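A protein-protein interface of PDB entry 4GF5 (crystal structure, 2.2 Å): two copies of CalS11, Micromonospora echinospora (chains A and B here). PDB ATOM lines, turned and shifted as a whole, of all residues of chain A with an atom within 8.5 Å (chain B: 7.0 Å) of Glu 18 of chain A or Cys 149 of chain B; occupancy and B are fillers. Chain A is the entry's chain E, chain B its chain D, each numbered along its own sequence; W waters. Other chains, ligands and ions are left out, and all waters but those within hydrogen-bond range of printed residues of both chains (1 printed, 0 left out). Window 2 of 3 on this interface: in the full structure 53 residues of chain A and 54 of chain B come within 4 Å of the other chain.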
ATOM      1  N   ASP A  15     -28.903  -5.380 -25.500  1.00  0.00           N
ATOM      2  CA  ASP A  15     -27.836  -5.505 -24.505  1.00  0.00           C
ATOM      3  C   ASP A  15     -27.587  -6.950 -24.069  1.00  0.00           C
ATOM      4  O   ASP A  15     -28.520  -7.691 -23.768  1.00  0.00           O
ATOM      5  CB  ASP A  15     -28.142  -4.670 -23.261  1.00  0.00           C
ATOM      6  CG  ASP A  15     -28.171  -3.183 -23.543  1.00  0.00           C
ATOM      7  OD1 ASP A  15     -27.577  -2.748 -24.552  1.00  0.00           O
ATOM      8  OD2 ASP A  15     -28.781  -2.442 -22.742  1.00  0.00           O
ATOM      9  N   SER A  16     -26.317  -7.334 -24.026  1.00  0.00           N
ATOM     10  CA  SER A  16     -25.922  -8.595 -23.429  1.00  0.00           C
ATOM     11  C   SER A  16     -26.237  -8.547 -21.937  1.00  0.00           C
ATOM     12  O   SER A  16     -26.425  -7.463 -21.367  1.00  0.00           O
ATOM     13  CB  SER A  16     -24.421  -8.811 -23.619  1.00  0.00           C
ATOM     14  OG  SER A  16     -23.679  -7.943 -22.780  1.00  0.00           O
ATOM     15  N   PRO A  17     -26.295  -9.724 -21.292  1.00  0.00           N
ATOM     16  CA  PRO A  17     -26.479  -9.748 -19.839  1.00  0.00           C
ATOM     17  C   PRO A  17     -25.397  -8.936 -19.135  1.00  0.00           C
ATOM     18  O   PRO A  17     -25.697  -8.212 -18.178  1.00  0.00           O
ATOM     19  CB  PRO A  17     -26.352 -11.233 -19.494  1.00  0.00           C
ATOM     20  CG  PRO A  17     -26.806 -11.936 -20.741  1.00  0.00           C
ATOM     21  CD  PRO A  17     -26.365 -11.073 -21.889  1.00  0.00           C
ATOM     22  N   GLU A  18     -24.164  -9.037 -19.615  1.00  0.00           N
ATOM     23  CA  GLU A  18     -23.059  -8.311 -18.993  1.00  0.00           C
ATOM     24  C   GLU A  18     -23.210  -6.805 -19.141  1.00  0.00           C
ATOM     25  O   GLU A  18     -22.890  -6.062 -18.214  1.00  0.00           O
ATOM     26  CB  GLU A  18     -21.702  -8.749 -19.542  1.00  0.00           C
ATOM     27  CG  GLU A  18     -21.308 -10.184 -19.207  1.00  0.00           C
ATOM     28  CD  GLU A  18     -21.969 -11.210 -20.122  1.00  0.00           C
ATOM     29  OE1 GLU A  18     -22.765 -10.814 -21.007  1.00  0.00           O
ATOM     30  OE2 GLU A  18     -21.691 -12.415 -19.957  1.00  0.00           O
ATOM     31  N   GLU A  19     -23.678  -6.359 -20.307  1.00  0.00           N
ATOM     32  CA  GLU A  19     -23.894  -4.926 -20.550  1.00  0.00           C
ATOM     33  C   GLU A  19     -24.978  -4.400 -19.613  1.00  0.00           C
ATOM     34  O   GLU A  19     -24.828  -3.343 -19.000  1.00  0.00           O
ATOM     35  CB  GLU A  19     -24.262  -4.663 -22.019  1.00  0.00           C
ATOM     36  CG  GLU A  19     -24.867  -3.288 -22.301  1.00  0.00           C
ATOM     37  CD  GLU A  19     -23.839  -2.159 -22.340  1.00  0.00           C
ATOM     38  OE1 GLU A  19     -22.620  -2.440 -22.205  1.00  0.00           O
ATOM     39  OE2 GLU A  19     -24.260  -0.988 -22.522  1.00  0.00           O
ATOM     40  N   THR A  20     -26.063  -5.159 -19.502  1.00  0.00           N
ATOM     41  CA  THR A  20     -27.124  -4.845 -18.558  1.00  0.00           C
ATOM     42  C   THR A  20     -26.555  -4.781 -17.146  1.00  0.00           C
ATOM     43  O   THR A  20     -26.868  -3.869 -16.383  1.00  0.00           O
ATOM     44  CB  THR A  20     -28.264  -5.886 -18.624  1.00  0.00           C
ATOM     45  OG1 THR A  20     -28.906  -5.811 -19.902  1.00  0.00           O
ATOM     46  CG2 THR A  20     -29.297  -5.625 -17.547  1.00  0.00           C
ATOM     47  N   GLU A  21     -25.695  -5.736 -16.812  1.00  0.00           N
ATOM     48  CA  GLU A  21     -25.101  -5.787 -15.477  1.00  0.00           C
ATOM     49  C   GLU A  21     -24.275  -4.537 -15.185  1.00  0.00           C
ATOM     50  O   GLU A  21     -24.428  -3.919 -14.123  1.00  0.00           O
ATOM     51  CB  GLU A  21     -24.264  -7.061 -15.300  1.00  0.00           C
ATOM     52  CG  GLU A  21     -23.601  -7.220 -13.938  1.00  0.00           C
ATOM     53  CD  GLU A  21     -24.593  -7.458 -12.795  1.00  0.00           C
ATOM     54  OE1 GLU A  21     -25.812  -7.593 -13.060  1.00  0.00           O
ATOM     55  OE2 GLU A  21     -24.145  -7.504 -11.623  1.00  0.00           O
ATOM     56  N   THR A  22     -23.412  -4.166 -16.135  1.00  0.00           N
ATOM     57  CA  THR A  22     -22.582  -2.970 -16.012  1.00  0.00           C
ATOM     58  C   THR A  22     -23.424  -1.717 -15.749  1.00  0.00           C
ATOM     59  O   THR A  22     -23.147  -0.947 -14.833  1.00  0.00           O
ATOM     60  CB  THR A  22     -21.709  -2.755 -17.267  1.00  0.00           C
ATOM     61  OG1 THR A  22     -20.737  -3.803 -17.353  1.00  0.00           O
ATOM     62  CG2 THR A  22     -20.976  -1.437 -17.179  1.00  0.00           C
ATOM     63  N   THR A  23     -24.464  -1.543 -16.557  1.00  0.00           N
ATOM     64  CA  THR A  23     -25.327  -0.384 -16.469  1.00  0.00           C
ATOM     65  C   THR A  23     -25.955  -0.296 -15.082  1.00  0.00           C
ATOM     66  O   THR A  23     -25.833   0.728 -14.412  1.00  0.00           O
ATOM     67  CB  THR A  23     -26.415  -0.421 -17.573  1.00  0.00           C
ATOM     68  OG1 THR A  23     -25.793  -0.675 -18.835  1.00  0.00           O
ATOM     69  CG2 THR A  23     -27.172   0.896 -17.650  1.00  0.00           C
ATOM     70  N   GLN A  24     -26.599  -1.377 -14.643  1.00  0.00           N
ATOM     71  CA  GLN A  24     -27.262  -1.390 -13.338  1.00  0.00           C
ATOM     72  C   GLN A  24     -26.304  -1.152 -12.187  1.00  0.00           C
ATOM     73  O   GLN A  24     -26.597  -0.373 -11.277  1.00  0.00           O
ATOM     74  CB  GLN A  24     -28.012  -2.700 -13.121  1.00  0.00           C
ATOM     75  CG  GLN A  24     -29.359  -2.737 -13.811  1.00  0.00           C
ATOM     76  CD  GLN A  24     -29.906  -4.144 -13.922  1.00  0.00           C
ATOM     77  OE1 GLN A  24     -29.355  -5.080 -13.339  1.00  0.00           O
ATOM     78  NE2 GLN A  24     -30.984  -4.306 -14.681  1.00  0.00           N
ATOM     79  N   ARG A  25     -25.156  -1.816 -12.232  1.00  0.00           N
ATOM     80  CA  ARG A  25     -24.143  -1.644 -11.198  1.00  0.00           C
ATOM     81  C   ARG A  25     -23.657  -0.198 -11.099  1.00  0.00           C
ATOM     82  O   ARG A  25     -23.563   0.352  -9.994  1.00  0.00           O
ATOM     83  CB  ARG A  25     -22.946  -2.559 -11.449  1.00  0.00           C
ATOM     84  CG  ARG A  25     -23.165  -4.023 -11.093  1.00  0.00           C
ATOM     85  CD  ARG A  25     -21.813  -4.714 -10.966  1.00  0.00           C
ATOM     86  NE  ARG A  25     -21.889  -6.170 -11.053  1.00  0.00           N
ATOM     87  CZ  ARG A  25     -20.824  -6.966 -11.022  1.00  0.00           C
ATOM     88  NH1 ARG A  25     -19.606  -6.438 -10.909  1.00  0.00           N
ATOM     89  NH2 ARG A  25     -20.973  -8.284 -11.104  1.00  0.00           N
ATOM     90  N   ARG A  49     -19.779   4.249 -19.067  1.00  0.00           N
ATOM     91  CA  ARG A  49     -19.320   2.991 -19.662  1.00  0.00           C
ATOM     92  C   ARG A  49     -18.942   3.108 -21.151  1.00  0.00           C
ATOM     93  O   ARG A  49     -19.363   4.045 -21.824  1.00  0.00           O
ATOM     94  CB  ARG A  49     -20.385   1.913 -19.480  1.00  0.00           C
ATOM     95  CG  ARG A  49     -21.606   2.063 -20.382  1.00  0.00           C
ATOM     96  CD  ARG A  49     -22.675   1.050 -19.985  1.00  0.00           C
ATOM     97  NE  ARG A  49     -23.836   1.086 -20.864  1.00  0.00           N
ATOM     98  CZ  ARG A  49     -24.835   1.960 -20.756  1.00  0.00           C
ATOM     99  NH1 ARG A  49     -24.807   2.894 -19.809  1.00  0.00           N
ATOM    100  NH2 ARG A  49     -25.859   1.909 -21.607  1.00  0.00           N
ATOM    101  N   LEU B 144     -14.534   0.110 -11.022  1.00  0.00           N
ATOM    102  CA  LEU B 144     -13.702  -0.538 -12.031  1.00  0.00           C
ATOM    103  C   LEU B 144     -14.188  -1.943 -12.392  1.00  0.00           C
ATOM    104  O   LEU B 144     -14.282  -2.281 -13.578  1.00  0.00           O
ATOM    105  CB  LEU B 144     -12.228  -0.546 -11.609  1.00  0.00           C
ATOM    106  CG  LEU B 144     -11.685   0.884 -11.452  1.00  0.00           C
ATOM    107  CD1 LEU B 144     -10.211   0.899 -11.092  1.00  0.00           C
ATOM    108  CD2 LEU B 144     -11.959   1.699 -12.716  1.00  0.00           C
ATOM    109  N   ASP B 145     -14.527  -2.751 -11.388  1.00  0.00           N
ATOM    110  CA  ASP B 145     -15.037  -4.086 -11.671  1.00  0.00           C
ATOM    111  C   ASP B 145     -16.297  -4.021 -12.528  1.00  0.00           C
ATOM    112  O   ASP B 145     -16.508  -4.863 -13.404  1.00  0.00           O
ATOM    113  CB  ASP B 145     -15.349  -4.851 -10.381  1.00  0.00           C
ATOM    114  CG  ASP B 145     -14.100  -5.313  -9.653  1.00  0.00           C
ATOM    115  OD1 ASP B 145     -13.055  -5.532 -10.305  1.00  0.00           O
ATOM    116  OD2 ASP B 145     -14.173  -5.462  -8.419  1.00  0.00           O
ATOM    117  N   ALA B 146     -17.136  -3.024 -12.261  1.00  0.00           N
ATOM    118  CA  ALA B 146     -18.414  -2.888 -12.947  1.00  0.00           C
ATOM    119  C   ALA B 146     -18.193  -2.651 -14.438  1.00  0.00           C
ATOM    120  O   ALA B 146     -18.855  -3.282 -15.278  1.00  0.00           O
ATOM    121  CB  ALA B 146     -19.239  -1.764 -12.332  1.00  0.00           C
ATOM    122  N   HIS B 147     -17.253  -1.762 -14.765  1.00  0.00           N
ATOM    123  CA  HIS B 147     -16.819  -1.590 -16.159  1.00  0.00           C
ATOM    124  C   HIS B 147     -16.317  -2.912 -16.787  1.00  0.00           C
ATOM    125  O   HIS B 147     -16.747  -3.294 -17.870  1.00  0.00           O
ATOM    126  CB  HIS B 147     -15.705  -0.539 -16.271  1.00  0.00           C
ATOM    127  CG  HIS B 147     -16.168   0.878 -16.099  1.00  0.00           C
ATOM    128  ND1 HIS B 147     -16.588   1.657 -17.156  1.00  0.00           N
ATOM    129  CD2 HIS B 147     -16.242   1.667 -14.998  1.00  0.00           C
ATOM    130  CE1 HIS B 147     -16.908   2.862 -16.715  1.00  0.00           C
ATOM    131  NE2 HIS B 147     -16.709   2.894 -15.408  1.00  0.00           N
ATOM    132  N   GLU B 148     -15.402  -3.595 -16.104  1.00  0.00           N
ATOM    133  CA  GLU B 148     -14.729  -4.772 -16.666  1.00  0.00           C
ATOM    134  C   GLU B 148     -15.643  -5.971 -16.867  1.00  0.00           C
ATOM    135  O   GLU B 148     -15.391  -6.825 -17.716  1.00  0.00           O
ATOM    136  CB  GLU B 148     -13.564  -5.179 -15.781  1.00  0.00           C
ATOM    137  CG  GLU B 148     -12.421  -4.202 -15.829  1.00  0.00           C
ATOM    138  CD  GLU B 148     -11.337  -4.546 -14.844  1.00  0.00           C
ATOM    139  OE1 GLU B 148     -11.541  -5.489 -14.036  1.00  0.00           O
ATOM    140  OE2 GLU B 148     -10.280  -3.877 -14.884  1.00  0.00           O
ATOM    141  N   CYS B 149     -16.701  -6.020 -16.076  1.00  0.00           N
ATOM    142  CA  CYS B 149     -17.696  -7.077 -16.151  1.00  0.00           C
ATOM    143  C   CYS B 149     -18.199  -7.331 -17.584  1.00  0.00           C
ATOM    144  O   CYS B 149     -18.621  -8.444 -17.915  1.00  0.00           O
ATOM    145  CB  CYS B 149     -18.852  -6.730 -15.199  1.00  0.00           C
ATOM    146  SG  CYS B 149     -20.443  -7.438 -15.624  1.00  0.00           S
ATOM    147  N   SER B 150     -18.139  -6.309 -18.438  1.00  0.00           N
ATOM    148  CA  SER B 150     -18.605  -6.454 -19.825  1.00  0.00           C
ATOM    149  C   SER B 150     -17.509  -6.207 -20.857  1.00  0.00           C
ATOM    150  O   SER B 150     -17.795  -5.957 -22.031  1.00  0.00           O
ATOM    151  CB  SER B 150     -19.817  -5.558 -20.115  1.00  0.00           C
ATOM    152  OG  SER B 150     -19.500  -4.190 -19.972  1.00  0.00           O
ATOM    153  N   ASP B 151     -16.257  -6.264 -20.424  1.00  0.00           N
ATOM    154  CA  ASP B 151     -15.154  -6.271 -21.372  1.00  0.00           C
ATOM    155  C   ASP B 151     -15.076  -7.653 -22.023  1.00  0.00           C
ATOM    156  O   ASP B 151     -15.460  -8.662 -21.419  1.00  0.00           O
ATOM    157  CB  ASP B 151     -13.824  -5.944 -20.691  1.00  0.00           C
ATOM    158  CG  ASP B 151     -13.671  -4.464 -20.370  1.00  0.00           C
ATOM    159  OD1 ASP B 151     -14.357  -3.611 -20.993  1.00  0.00           O
ATOM    160  OD2 ASP B 151     -12.847  -4.153 -19.484  1.00  0.00           O
ATOM    161  N   PHE B 152     -14.582  -7.693 -23.255  1.00  0.00           N
ATOM    162  CA  PHE B 152     -14.367  -8.955 -23.946  1.00  0.00           C
ATOM    163  C   PHE B 152     -13.472  -9.875 -23.112  1.00  0.00           C
ATOM    164  O   PHE B 152     -13.682 -11.085 -23.083  1.00  0.00           O
ATOM    165  CB  PHE B 152     -13.760  -8.714 -25.334  1.00  0.00           C
ATOM    166  CG  PHE B 152     -13.641  -9.964 -26.166  1.00  0.00           C
ATOM    167  CD1 PHE B 152     -12.485 -10.728 -26.133  1.00  0.00           C
ATOM    168  CD2 PHE B 152     -14.696 -10.381 -26.969  1.00  0.00           C
ATOM    169  CE1 PHE B 152     -12.373 -11.891 -26.896  1.00  0.00           C
ATOM    170  CE2 PHE B 152     -14.598 -11.530 -27.723  1.00  0.00           C
ATOM    171  CZ  PHE B 152     -13.429 -12.289 -27.690  1.00  0.00           C
ATOM    172  N   GLY B 154     -13.236  -9.777 -19.821  1.00  0.00           N
ATOM    173  CA  GLY B 154     -13.729  -9.601 -18.468  1.00  0.00           C
ATOM    174  C   GLY B 154     -13.406 -10.741 -17.521  1.00  0.00           C
ATOM    175  O   GLY B 154     -13.312 -10.541 -16.316  1.00  0.00           O
ATOM    176  N   HIS B 155     -13.199 -11.935 -18.067  1.00  0.00           N
ATOM    177  CA  HIS B 155     -12.917 -13.113 -17.252  1.00  0.00           C
ATOM    178  C   HIS B 155     -11.484 -13.132 -16.728  1.00  0.00           C
ATOM    179  O   HIS B 155     -11.142 -13.927 -15.853  1.00  0.00           O
ATOM    180  CB  HIS B 155     -13.180 -14.377 -18.067  1.00  0.00           C
ATOM    181  CG  HIS B 155     -12.396 -14.443 -19.339  1.00  0.00           C
ATOM    182  ND1 HIS B 155     -12.785 -13.788 -20.490  1.00  0.00           N
ATOM    183  CD2 HIS B 155     -11.238 -15.081 -19.641  1.00  0.00           C
ATOM    184  CE1 HIS B 155     -11.909 -14.032 -21.450  1.00  0.00           C
ATOM    185  NE2 HIS B 155     -10.962 -14.815 -20.964  1.00  0.00           N
ATOM    186  N   ARG B 159      -6.904  -6.658 -14.123  1.00  0.00           N
ATOM    187  CA  ARG B 159      -6.718  -5.757 -15.255  1.00  0.00           C
ATOM    188  C   ARG B 159      -6.786  -4.294 -14.782  1.00  0.00           C
ATOM    189  O   ARG B 159      -6.249  -3.381 -15.426  1.00  0.00           O
ATOM    190  CB  ARG B 159      -7.710  -6.093 -16.367  1.00  0.00           C
ATOM    191  CG  ARG B 159      -7.418  -7.457 -17.000  1.00  0.00           C
ATOM    192  CD  ARG B 159      -8.503  -7.881 -17.961  1.00  0.00           C
ATOM    193  NE  ARG B 159      -8.912  -6.757 -18.779  1.00  0.00           N
ATOM    194  CZ  ARG B 159     -10.130  -6.240 -18.802  1.00  0.00           C
ATOM    195  NH1 ARG B 159     -10.363  -5.204 -19.591  1.00  0.00           N
ATOM    196  NH2 ARG B 159     -11.110  -6.755 -18.061  1.00  0.00           N
HETATM  197  O   HOH W   1     -18.861  -3.867  -9.511  1.00  0.00           O
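Among the printed residues, pairs that only touch across the chains: Glu 18 of chain A with Cys 149 of chain B, Glu 21 of chain A with Cys 149 of chain B, Glu 18 of chain A with Ser 150 of chain B, Arg 49 of chain A with His 147 of chain B, Arg 25 of chain A with Ala 146 of chain B and Glu 19 of chain A with Ser 150 of chain B.
Water W1 lies within hydrogen-bond range of the guanidinium group of Arg 25 of chain A (3.0 Å) and the backbone NH of Ala 146 of chain B (3.4 Å).
Of the printed residues of chain B, Glu 19 of chain A touches Ser 150 (3.9 Å). Printed residues of chain A within 4 Å of His 147 of chain B: Arg 49. Printed residues of chain A within 4 Å of Ser 150 of chain B: Glu 18 (3.6 Å), Glu 19 (3.9 Å) and Thr 22 (2.9 Å).
N of Glu 18 of chain A lies close to OG of Ser 16 of chain A (3.4 Å). The side-chain hydroxyl (OG) of Ser 16 of chain A is in hydrogen-bond range of the backbone NH (N) of Glu 19 of chain A (2.9 Å). The side-chain hydroxyl of Thr 22 of chain A sits at hydrogen-bond distance from the backbone carbonyl oxygen of Glu 18 of chain A, 3.2 Å away. NE of Arg 49 of chain A is in salt-bridge range of OE2 of Glu 19 of chain A (2.7 Å). The guanidinium group of Arg 25 of chain A lies within salt-bridge range of the side-chain carboxylate of Glu 21 of chain A (2.7 Å). OG1 of Thr 23 of chain A sits at hydrogen-bond distance from NE of Arg 49 of chain A (3.3 Å).
No position is printed for both chains. Of the 8 pairs that touch across the chains among the printed residues, none has its exchanged pair printed and touching as well.
Hydrophobic or aromatic side chains of chain B that line the printed part of chain A: Ala 146 and His 147.
OG1 of Thr 22 of chain A sits at hydrogen-bond distance from O of Ala 146 of chain B, 2.8 Å away. The side-chain hydroxyl (OG1) of Thr 22 of chain A lies within hydrogen-bond range of the side-chain hydroxyl (OG) of Ser 150 of chain B.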
